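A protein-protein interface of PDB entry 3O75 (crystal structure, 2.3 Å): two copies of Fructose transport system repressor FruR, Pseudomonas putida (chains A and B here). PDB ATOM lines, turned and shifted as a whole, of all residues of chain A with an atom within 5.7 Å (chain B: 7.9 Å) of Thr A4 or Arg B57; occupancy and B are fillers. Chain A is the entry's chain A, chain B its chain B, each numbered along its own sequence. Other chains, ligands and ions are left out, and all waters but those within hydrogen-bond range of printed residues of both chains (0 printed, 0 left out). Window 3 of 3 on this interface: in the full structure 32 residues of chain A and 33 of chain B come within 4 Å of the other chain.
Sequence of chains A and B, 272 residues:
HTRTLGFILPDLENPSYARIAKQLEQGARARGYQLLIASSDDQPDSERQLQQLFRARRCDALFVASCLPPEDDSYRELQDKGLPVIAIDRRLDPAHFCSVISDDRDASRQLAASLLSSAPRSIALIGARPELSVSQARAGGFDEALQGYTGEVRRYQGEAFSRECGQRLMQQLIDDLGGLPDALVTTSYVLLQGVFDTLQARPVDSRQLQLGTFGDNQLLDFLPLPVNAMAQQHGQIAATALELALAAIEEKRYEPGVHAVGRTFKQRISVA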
ATOM      1  N   THR A   2      17.705 -16.576   8.666  1.00  0.00           N
ATOM      2  CA  THR A   2      16.835 -16.289   9.801  1.00  0.00           C
ATOM      3  C   THR A   2      17.620 -15.849  11.032  1.00  0.00           C
ATOM      4  O   THR A   2      17.050 -15.312  11.981  1.00  0.00           O
ATOM      5  CB  THR A   2      15.956 -17.502  10.168  1.00  0.00           C
ATOM      6  OG1 THR A   2      16.785 -18.579  10.621  1.00  0.00           O
ATOM      7  CG2 THR A   2      15.147 -17.954   8.962  1.00  0.00           C
ATOM      8  N   ARG A   3      18.930 -16.078  11.010  1.00  0.00           N
ATOM      9  CA  ARG A   3      19.794 -15.747  12.141  1.00  0.00           C
ATOM     10  C   ARG A   3      19.393 -16.485  13.417  1.00  0.00           C
ATOM     11  O   ARG A   3      19.697 -16.046  14.527  1.00  0.00           O
ATOM     12  CB  ARG A   3      19.834 -14.236  12.375  1.00  0.00           C
ATOM     13  CG  ARG A   3      21.058 -13.562  11.784  1.00  0.00           C
ATOM     14  CD  ARG A   3      21.260 -13.961  10.331  1.00  0.00           C
ATOM     15  NE  ARG A   3      22.673 -14.115  10.001  1.00  0.00           N
ATOM     16  CZ  ARG A   3      23.197 -13.872   8.804  1.00  0.00           C
ATOM     17  NH1 ARG A   3      22.425 -13.451   7.810  1.00  0.00           N
ATOM     18  NH2 ARG A   3      24.497 -14.042   8.600  1.00  0.00           N
ATOM     19  N   THR A   4      18.705 -17.608  13.250  1.00  0.00           N
ATOM     20  CA  THR A   4      18.368 -18.462  14.379  1.00  0.00           C
ATOM     21  C   THR A   4      18.992 -19.840  14.197  1.00  0.00           C
ATOM     22  O   THR A   4      19.218 -20.294  13.070  1.00  0.00           O
ATOM     23  CB  THR A   4      16.839 -18.605  14.556  1.00  0.00           C
ATOM     24  OG1 THR A   4      16.296 -19.382  13.482  1.00  0.00           O
ATOM     25  CG2 THR A   4      16.171 -17.233  14.577  1.00  0.00           C
ATOM     26  N   LEU A   5      19.276 -20.499  15.314  1.00  0.00           N
ATOM     27  CA  LEU A   5      19.799 -21.855  15.295  1.00  0.00           C
ATOM     28  C   LEU A   5      18.931 -22.711  16.204  1.00  0.00           C
ATOM     29  O   LEU A   5      18.363 -22.212  17.176  1.00  0.00           O
ATOM     30  CB  LEU A   5      21.254 -21.877  15.770  1.00  0.00           C
ATOM     31  CG  LEU A   5      22.255 -21.068  14.938  1.00  0.00           C
ATOM     32  CD1 LEU A   5      23.617 -21.027  15.612  1.00  0.00           C
ATOM     33  CD2 LEU A   5      22.376 -21.627  13.530  1.00  0.00           C
ATOM     34  N   GLY A   6      18.813 -23.994  15.880  1.00  0.00           N
ATOM     35  CA  GLY A   6      18.008 -24.905  16.674  1.00  0.00           C
ATOM     36  C   GLY A   6      18.853 -25.944  17.381  1.00  0.00           C
ATOM     37  O   GLY A   6      19.913 -26.333  16.889  1.00  0.00           O
ATOM     38  N   TYR A  33      23.459 -14.525  16.377  1.00  0.00           N
ATOM     39  CA  TYR A  33      22.446 -15.560  16.200  1.00  0.00           C
ATOM     40  C   TYR A  33      21.642 -15.808  17.471  1.00  0.00           C
ATOM     41  O   TYR A  33      22.148 -15.638  18.582  1.00  0.00           O
ATOM     42  CB  TYR A  33      23.091 -16.870  15.762  1.00  0.00           C
ATOM     43  CG  TYR A  33      23.463 -16.946  14.301  1.00  0.00           C
ATOM     44  CD1 TYR A  33      24.696 -16.484  13.854  1.00  0.00           C
ATOM     45  CD2 TYR A  33      22.595 -17.504  13.371  1.00  0.00           C
ATOM     46  CE1 TYR A  33      25.050 -16.565  12.519  1.00  0.00           C
ATOM     47  CE2 TYR A  33      22.939 -17.589  12.033  1.00  0.00           C
ATOM     48  CZ  TYR A  33      24.170 -17.120  11.614  1.00  0.00           C
ATOM     49  OH  TYR A  33      24.525 -17.202  10.287  1.00  0.00           O
ATOM     50  N   GLN A  34      20.390 -16.221  17.298  1.00  0.00           N
ATOM     51  CA  GLN A  34      19.551 -16.629  18.420  1.00  0.00           C
ATOM     52  C   GLN A  34      19.450 -18.152  18.447  1.00  0.00           C
ATOM     53  O   GLN A  34      19.585 -18.801  17.413  1.00  0.00           O
ATOM     54  CB  GLN A  34      18.161 -15.996  18.305  1.00  0.00           C
ATOM     55  CG  GLN A  34      17.693 -15.269  19.553  1.00  0.00           C
ATOM     56  CD  GLN A  34      18.452 -13.981  19.817  1.00  0.00           C
ATOM     57  OE1 GLN A  34      18.796 -13.250  18.892  1.00  0.00           O
ATOM     58  NE2 GLN A  34      18.703 -13.692  21.092  1.00  0.00           N
ATOM     59  N   LEU A  35      19.206 -18.720  19.625  1.00  0.00           N
ATOM     60  CA  LEU A  35      19.129 -20.172  19.773  1.00  0.00           C
ATOM     61  C   LEU A  35      17.801 -20.635  20.364  1.00  0.00           C
ATOM     62  O   LEU A  35      17.436 -20.256  21.482  1.00  0.00           O
ATOM     63  CB  LEU A  35      20.278 -20.690  20.645  1.00  0.00           C
ATOM     64  CG  LEU A  35      20.335 -22.209  20.865  1.00  0.00           C
ATOM     65  CD1 LEU A  35      20.573 -22.955  19.552  1.00  0.00           C
ATOM     66  CD2 LEU A  35      21.398 -22.584  21.884  1.00  0.00           C
ATOM     67  N   LEU A  36      17.091 -21.466  19.606  1.00  0.00           N
ATOM     68  CA  LEU A  36      15.860 -22.090  20.074  1.00  0.00           C
ATOM     69  C   LEU A  36      16.107 -23.541  20.469  1.00  0.00           C
ATOM     70  O   LEU A  36      16.639 -24.327  19.685  1.00  0.00           O
ATOM     71  CB  LEU A  36      14.792 -22.029  18.988  1.00  0.00           C
ATOM     72  CG  LEU A  36      14.239 -20.642  18.667  1.00  0.00           C
ATOM     73  CD1 LEU A  36      13.186 -20.744  17.583  1.00  0.00           C
ATOM     74  CD2 LEU A  36      13.655 -20.024  19.918  1.00  0.00           C
ATOM     75  N   ARG A  57      10.309 -23.709  11.174  1.00  0.00           N
ATOM     76  CA  ARG A  57      10.909 -22.498  11.713  1.00  0.00           C
ATOM     77  C   ARG A  57      12.028 -22.054  10.779  1.00  0.00           C
ATOM     78  O   ARG A  57      12.534 -20.938  10.881  1.00  0.00           O
ATOM     79  CB  ARG A  57      11.481 -22.770  13.107  1.00  0.00           C
ATOM     80  CG  ARG A  57      10.947 -21.868  14.207  1.00  0.00           C
ATOM     81  CD  ARG A  57       9.662 -22.415  14.828  1.00  0.00           C
ATOM     82  NE  ARG A  57       8.619 -22.684  13.839  1.00  0.00           N
ATOM     83  CZ  ARG A  57       7.313 -22.646  14.097  1.00  0.00           C
ATOM     84  NH1 ARG A  57       6.883 -22.335  15.313  1.00  0.00           N
ATOM     85  NH2 ARG A  57       6.435 -22.909  13.136  1.00  0.00           N
ATOM     86  N   ARG A  58      12.401 -22.947   9.866  1.00  0.00           N
ATOM     87  CA  ARG A  58      13.555 -22.754   8.988  1.00  0.00           C
ATOM     88  C   ARG A  58      14.728 -22.054   9.671  1.00  0.00           C
ATOM     89  O   ARG A  58      15.169 -20.989   9.235  1.00  0.00           O
ATOM     90  CB  ARG A  58      13.173 -22.053   7.678  1.00  0.00           C
ATOM     91  CG  ARG A  58      12.946 -23.020   6.519  1.00  0.00           C
ATOM     92  CD  ARG A  58      13.719 -22.616   5.268  1.00  0.00           C
ATOM     93  NE  ARG A  58      15.164 -22.562   5.487  1.00  0.00           N
ATOM     94  CZ  ARG A  58      15.997 -23.582   5.295  1.00  0.00           C
ATOM     95  NH1 ARG A  58      15.539 -24.755   4.879  1.00  0.00           N
ATOM     96  NH2 ARG A  58      17.296 -23.429   5.520  1.00  0.00           N
ATOM     97  N   CYS A  59      15.220 -22.659  10.747  1.00  0.00           N
ATOM     98  CA  CYS A  59      16.446 -22.202  11.381  1.00  0.00           C
ATOM     99  C   CYS A  59      17.595 -22.397  10.398  1.00  0.00           C
ATOM    100  O   CYS A  59      17.517 -23.249   9.510  1.00  0.00           O
ATOM    101  CB  CYS A  59      16.700 -22.980  12.672  1.00  0.00           C
ATOM    102  SG  CYS A  59      15.467 -22.684  13.974  1.00  0.00           S
ATOM    103  N   ASP A  60      18.648 -21.599  10.545  1.00  0.00           N
ATOM    104  CA  ASP A  60      19.789 -21.671   9.636  1.00  0.00           C
ATOM    105  C   ASP A  60      20.524 -23.006   9.753  1.00  0.00           C
ATOM    106  O   ASP A  60      20.923 -23.592   8.747  1.00  0.00           O
ATOM    107  CB  ASP A  60      20.757 -20.514   9.883  1.00  0.00           C
ATOM    108  CG  ASP A  60      20.206 -19.182   9.414  1.00  0.00           C
ATOM    109  OD1 ASP A  60      19.037 -19.133   8.980  1.00  0.00           O
ATOM    110  OD2 ASP A  60      20.948 -18.180   9.482  1.00  0.00           O
ATOM    111  N   ALA A  61      20.700 -23.481  10.983  1.00  0.00           N
ATOM    112  CA  ALA A  61      21.343 -24.769  11.220  1.00  0.00           C
ATOM    113  C   ALA A  61      20.748 -25.442  12.452  1.00  0.00           C
ATOM    114  O   ALA A  61      20.132 -24.784  13.287  1.00  0.00           O
ATOM    115  CB  ALA A  61      22.850 -24.597  11.374  1.00  0.00           C
ATOM    116  N   HIS B   1      -2.771 -20.222  14.312  1.00  0.00           N
ATOM    117  CA  HIS B   1      -2.195 -21.283  15.132  1.00  0.00           C
ATOM    118  C   HIS B   1      -0.872 -21.813  14.577  1.00  0.00           C
ATOM    119  O   HIS B   1      -0.580 -21.677  13.390  1.00  0.00           O
ATOM    120  CB  HIS B   1      -3.187 -22.440  15.290  1.00  0.00           C
ATOM    121  CG  HIS B   1      -4.058 -22.329  16.501  1.00  0.00           C
ATOM    122  ND1 HIS B   1      -4.948 -21.295  16.687  1.00  0.00           N
ATOM    123  CD2 HIS B   1      -4.185 -23.133  17.586  1.00  0.00           C
ATOM    124  CE1 HIS B   1      -5.581 -21.459  17.835  1.00  0.00           C
ATOM    125  NE2 HIS B   1      -5.135 -22.569  18.400  1.00  0.00           N
ATOM    126  N   THR B   2      -0.083 -22.416  15.459  1.00  0.00           N
ATOM    127  CA  THR B   2       1.140 -23.113  15.082  1.00  0.00           C
ATOM    128  C   THR B   2       1.281 -24.359  15.942  1.00  0.00           C
ATOM    129  O   THR B   2       2.077 -25.246  15.642  1.00  0.00           O
ATOM    130  CB  THR B   2       2.397 -22.238  15.269  1.00  0.00           C
ATOM    131  OG1 THR B   2       2.311 -21.524  16.509  1.00  0.00           O
ATOM    132  CG2 THR B   2       2.542 -21.251  14.120  1.00  0.00           C
ATOM    133  N   THR B   4       2.567 -24.472  18.767  1.00  0.00           N
ATOM    134  CA  THR B   4       3.809 -24.407  19.522  1.00  0.00           C
ATOM    135  C   THR B   4       3.763 -23.290  20.558  1.00  0.00           C
ATOM    136  O   THR B   4       3.223 -22.212  20.310  1.00  0.00           O
ATOM    137  CB  THR B   4       5.033 -24.215  18.604  1.00  0.00           C
ATOM    138  OG1 THR B   4       5.067 -22.867  18.118  1.00  0.00           O
ATOM    139  CG2 THR B   4       4.975 -25.185  17.433  1.00  0.00           C
ATOM    140  N   LEU B  36       9.118 -24.408  22.432  1.00  0.00           N
ATOM    141  CA  LEU B  36      10.399 -23.859  22.005  1.00  0.00           C
ATOM    142  C   LEU B  36      10.962 -22.975  23.111  1.00  0.00           C
ATOM    143  O   LEU B  36      10.312 -22.024  23.552  1.00  0.00           O
ATOM    144  CB  LEU B  36      10.246 -23.061  20.712  1.00  0.00           C
ATOM    145  CG  LEU B  36       9.818 -23.852  19.479  1.00  0.00           C
ATOM    146  CD1 LEU B  36       9.308 -22.924  18.387  1.00  0.00           C
ATOM    147  CD2 LEU B  36      10.966 -24.697  18.977  1.00  0.00           C
ATOM    148  N   LEU B  50      14.541 -11.827  21.873  1.00  0.00           N
ATOM    149  CA  LEU B  50      13.736 -13.044  21.859  1.00  0.00           C
ATOM    150  C   LEU B  50      12.251 -12.726  21.706  1.00  0.00           C
ATOM    151  O   LEU B  50      11.487 -13.526  21.169  1.00  0.00           O
ATOM    152  CB  LEU B  50      13.973 -13.855  23.131  1.00  0.00           C
ATOM    153  CG  LEU B  50      15.365 -14.463  23.287  1.00  0.00           C
ATOM    154  CD1 LEU B  50      15.551 -15.024  24.683  1.00  0.00           C
ATOM    155  CD2 LEU B  50      15.596 -15.542  22.231  1.00  0.00           C
ATOM    156  N   GLN B  51      11.853 -11.554  22.188  1.00  0.00           N
ATOM    157  CA  GLN B  51      10.469 -11.101  22.108  1.00  0.00           C
ATOM    158  C   GLN B  51      10.008 -11.056  20.660  1.00  0.00           C
ATOM    159  O   GLN B  51       8.994 -11.651  20.295  1.00  0.00           O
ATOM    160  CB  GLN B  51      10.355  -9.703  22.708  1.00  0.00           C
ATOM    161  CG  GLN B  51       9.239  -9.528  23.707  1.00  0.00           C
ATOM    162  CD  GLN B  51       9.142  -8.100  24.192  1.00  0.00           C
ATOM    163  OE1 GLN B  51       9.262  -7.162  23.405  1.00  0.00           O
ATOM    164  NE2 GLN B  51       8.931  -7.925  25.491  1.00  0.00           N
ATOM    165  N   GLN B  52      10.771 -10.344  19.838  1.00  0.00           N
ATOM    166  CA  GLN B  52      10.463 -10.213  18.425  1.00  0.00           C
ATOM    167  C   GLN B  52      10.532 -11.564  17.729  1.00  0.00           C
ATOM    168  O   GLN B  52       9.816 -11.806  16.760  1.00  0.00           O
ATOM    169  CB  GLN B  52      11.436  -9.241  17.765  1.00  0.00           C
ATOM    170  CG  GLN B  52      11.609  -7.937  18.524  1.00  0.00           C
ATOM    171  CD  GLN B  52      12.559  -6.984  17.828  1.00  0.00           C
ATOM    172  OE1 GLN B  52      12.868  -7.147  16.647  1.00  0.00           O
ATOM    173  NE2 GLN B  52      13.026  -5.977  18.558  1.00  0.00           N
ATOM    174  N   LEU B  53      11.400 -12.442  18.221  1.00  0.00           N
ATOM    175  CA  LEU B  53      11.561 -13.759  17.619  1.00  0.00           C
ATOM    176  C   LEU B  53      10.307 -14.611  17.796  1.00  0.00           C
ATOM    177  O   LEU B  53       9.730 -15.078  16.821  1.00  0.00           O
ATOM    178  CB  LEU B  53      12.783 -14.480  18.192  1.00  0.00           C
ATOM    179  CG  LEU B  53      13.026 -15.880  17.621  1.00  0.00           C
ATOM    180  CD1 LEU B  53      13.098 -15.827  16.104  1.00  0.00           C
ATOM    181  CD2 LEU B  53      14.289 -16.496  18.199  1.00  0.00           C
ATOM    182  N   PHE B  54       9.884 -14.811  19.038  1.00  0.00           N
ATOM    183  CA  PHE B  54       8.674 -15.589  19.290  1.00  0.00           C
ATOM    184  C   PHE B  54       7.439 -14.912  18.703  1.00  0.00           C
ATOM    185  O   PHE B  54       6.448 -15.574  18.392  1.00  0.00           O
ATOM    186  CB  PHE B  54       8.481 -15.845  20.784  1.00  0.00           C
ATOM    187  CG  PHE B  54       9.378 -16.909  21.333  1.00  0.00           C
ATOM    188  CD1 PHE B  54      10.387 -16.593  22.224  1.00  0.00           C
ATOM    189  CD2 PHE B  54       9.219 -18.230  20.946  1.00  0.00           C
ATOM    190  CE1 PHE B  54      11.213 -17.573  22.728  1.00  0.00           C
ATOM    191  CE2 PHE B  54      10.046 -19.215  21.444  1.00  0.00           C
ATOM    192  CZ  PHE B  54      11.045 -18.887  22.337  1.00  0.00           C
ATOM    193  N   ARG B  55       7.502 -13.594  18.550  1.00  0.00           N
ATOM    194  CA  ARG B  55       6.397 -12.853  17.957  1.00  0.00           C
ATOM    195  C   ARG B  55       6.265 -13.185  16.475  1.00  0.00           C
ATOM    196  O   ARG B  55       5.167 -13.448  15.984  1.00  0.00           O
ATOM    197  CB  ARG B  55       6.585 -11.349  18.158  1.00  0.00           C
ATOM    198  CG  ARG B  55       6.733 -10.564  16.868  1.00  0.00           C
ATOM    199  CD  ARG B  55       6.838  -9.073  17.135  1.00  0.00           C
ATOM    200  NE  ARG B  55       7.006  -8.315  15.900  1.00  0.00           N
ATOM    201  CZ  ARG B  55       7.055  -6.987  15.834  1.00  0.00           C
ATOM    202  NH1 ARG B  55       6.947  -6.261  16.939  1.00  0.00           N
ATOM    203  NH2 ARG B  55       7.210  -6.387  14.662  1.00  0.00           N
ATOM    204  N   ALA B  56       7.396 -13.182  15.772  1.00  0.00           N
ATOM    205  CA  ALA B  56       7.427 -13.464  14.341  1.00  0.00           C
ATOM    206  C   ALA B  56       7.233 -14.951  14.079  1.00  0.00           C
ATOM    207  O   ALA B  56       6.576 -15.341  13.114  1.00  0.00           O
ATOM    208  CB  ALA B  56       8.741 -12.984  13.737  1.00  0.00           C
ATOM    209  N   ARG B  57       7.810 -15.775  14.945  1.00  0.00           N
ATOM    210  CA  ARG B  57       7.676 -17.220  14.839  1.00  0.00           C
ATOM    211  C   ARG B  57       6.204 -17.600  14.965  1.00  0.00           C
ATOM    212  O   ARG B  57       5.801 -18.709  14.615  1.00  0.00           O
ATOM    213  CB  ARG B  57       8.495 -17.907  15.934  1.00  0.00           C
ATOM    214  CG  ARG B  57       9.343 -19.074  15.456  1.00  0.00           C
ATOM    215  CD  ARG B  57      10.779 -18.653  15.143  1.00  0.00           C
ATOM    216  NE  ARG B  57      10.884 -17.801  13.959  1.00  0.00           N
ATOM    217  CZ  ARG B  57      11.938 -17.778  13.147  1.00  0.00           C
ATOM    218  NH1 ARG B  57      12.977 -18.568  13.382  1.00  0.00           N
ATOM    219  NH2 ARG B  57      11.951 -16.970  12.095  1.00  0.00           N
ATOM    220  N   ARG B  58       5.410 -16.659  15.467  1.00  0.00           N
ATOM    221  CA  ARG B  58       3.975 -16.850  15.662  1.00  0.00           C
ATOM    222  C   ARG B  58       3.663 -18.104  16.476  1.00  0.00           C
ATOM    223  O   ARG B  58       2.930 -18.981  16.022  1.00  0.00           O
ATOM    224  CB  ARG B  58       3.232 -16.872  14.318  1.00  0.00           C
ATOM    225  CG  ARG B  58       1.772 -16.406  14.395  1.00  0.00           C
ATOM    226  CD  ARG B  58       0.891 -17.407  15.138  1.00  0.00           C
ATOM    227  NE  ARG B  58      -0.074 -16.782  16.045  1.00  0.00           N
ATOM    228  CZ  ARG B  58       0.218 -15.828  16.927  1.00  0.00           C
ATOM    229  NH1 ARG B  58       1.455 -15.357  17.031  1.00  0.00           N
ATOM    230  NH2 ARG B  58      -0.736 -15.338  17.708  1.00  0.00           N
ATOM    231  N   CYS B  59       4.238 -18.191  17.672  1.00  0.00           N
ATOM    232  CA  CYS B  59       3.841 -19.214  18.628  1.00  0.00           C
ATOM    233  C   CYS B  59       2.457 -18.854  19.157  1.00  0.00           C
ATOM    234  O   CYS B  59       2.079 -17.681  19.153  1.00  0.00           O
ATOM    235  CB  CYS B  59       4.851 -19.306  19.770  1.00  0.00           C
ATOM    236  SG  CYS B  59       6.471 -19.939  19.257  1.00  0.00           S
ATOM    237  N   ASP B  60       1.700 -19.853  19.599  1.00  0.00           N
ATOM    238  CA  ASP B  60       0.333 -19.622  20.055  1.00  0.00           C
ATOM    239  C   ASP B  60       0.288 -18.899  21.402  1.00  0.00           C
ATOM    240  O   ASP B  60      -0.599 -18.088  21.651  1.00  0.00           O
ATOM    241  CB  ASP B  60      -0.439 -20.939  20.136  1.00  0.00           C
ATOM    242  CG  ASP B  60      -0.567 -21.626  18.786  1.00  0.00           C
ATOM    243  OD1 ASP B  60      -0.187 -21.017  17.760  1.00  0.00           O
ATOM    244  OD2 ASP B  60      -1.047 -22.779  18.755  1.00  0.00           O
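The guanidinium group (NH1) of Arg B57 is in hydrogen-bond range of the side-chain hydroxyl (OG1) of Thr A4 (3.4 Å).
NH1 of Arg A57 is in hydrogen-bond range of OG1 of Thr B4 (3.4 Å).
The backbone carbonyl oxygen (O) of Arg A57 sits at hydrogen-bond distance from the guanidinium group (NH1) of Arg B57 (3.5 Å).
The side-chain hydroxyl of Thr A4 lies within hydrogen-bond range of the side-chain hydroxyl of Thr A2, at 3.0 Å.
The backbone carbonyl oxygen (O) of Arg A3 lies within hydrogen-bond range of the backbone NH (N) of Gln A34.
O of Thr A4 sits at hydrogen-bond distance from N of Asp A60 (2.9 Å).
The backbone carbonyl oxygen (O) of Leu A5 is in hydrogen-bond range of the backbone NH (N) of Leu A36 (2.8 Å).
OG1 of Thr B4 is in hydrogen-bond range of SG of Cys B59.
O of Phe B54 sits close to N of Cys B59, 3.5 Å away.
Among the printed residues, pairs that only touch across the chains: Thr A4 with Leu B53 (3.7 Å), Gln A34 with Leu B50 (3.4 Å), Gln A34 with Leu B53 (3.9 Å), Leu A36 with Leu B53 (3.98 Å), Leu A36 with Phe B54 (3.7 Å) and Arg A57 with Leu B36 (3.6 Å).
Of chain B, only Leu B53 (3.7 Å) and Arg B57 (3.4 Å) come within 4 Å of Thr A4.
Of the printed residues of chain A, Arg B57 touches Thr A4 (3.4 Å) and Arg A57 (3.4 Å).
Printed residues of chain A within 4 Å of Leu B50: Gln A34 (3.4 Å).
Of the printed residues of chain A, Leu B53 touches Thr A4, Gln A34 and Leu A36.
Of the printed residues of chain A, Thr B4 touches Arg A57.
Of the printed residues of chain A, Leu B36 touches Arg A57.
Of the printed residues of chain B, Arg A57 touches Thr B4, Leu B36 and Arg B57.
The nearest printed residue of chain B that does not touch Thr A4 is Leu B50 (7.9 Å).
The nearest printed residue of chain A that does not touch Thr B4 is Leu A36 (8.4 Å).
Hydrophobic or aromatic side chains of chain A that line the printed part of chain B: Leu A36.
Along chain A the printed residues that touch a printed residue of chain B span positions 4 to 57.
Of the 15 printed residues of chain B, 6 touch a printed residue of chain A.
Printed residues of chain B that touch a printed residue of chain A: Thr B4, Leu B36, Leu B50, Leu B53, Phe B54 and Arg B57.
Among the printed residues, 9 pairs touch across the chains.
Thr A4 touches Arg B57, and with the chains exchanged Arg A57 touches Thr B4.
Arg A57 touches Leu B36, but with the chains exchanged Leu A36 does not touch Arg B57 (4.01 Å).
Arg B57 touches its own counterpart, Arg A57.
7 positions are printed for both chains.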
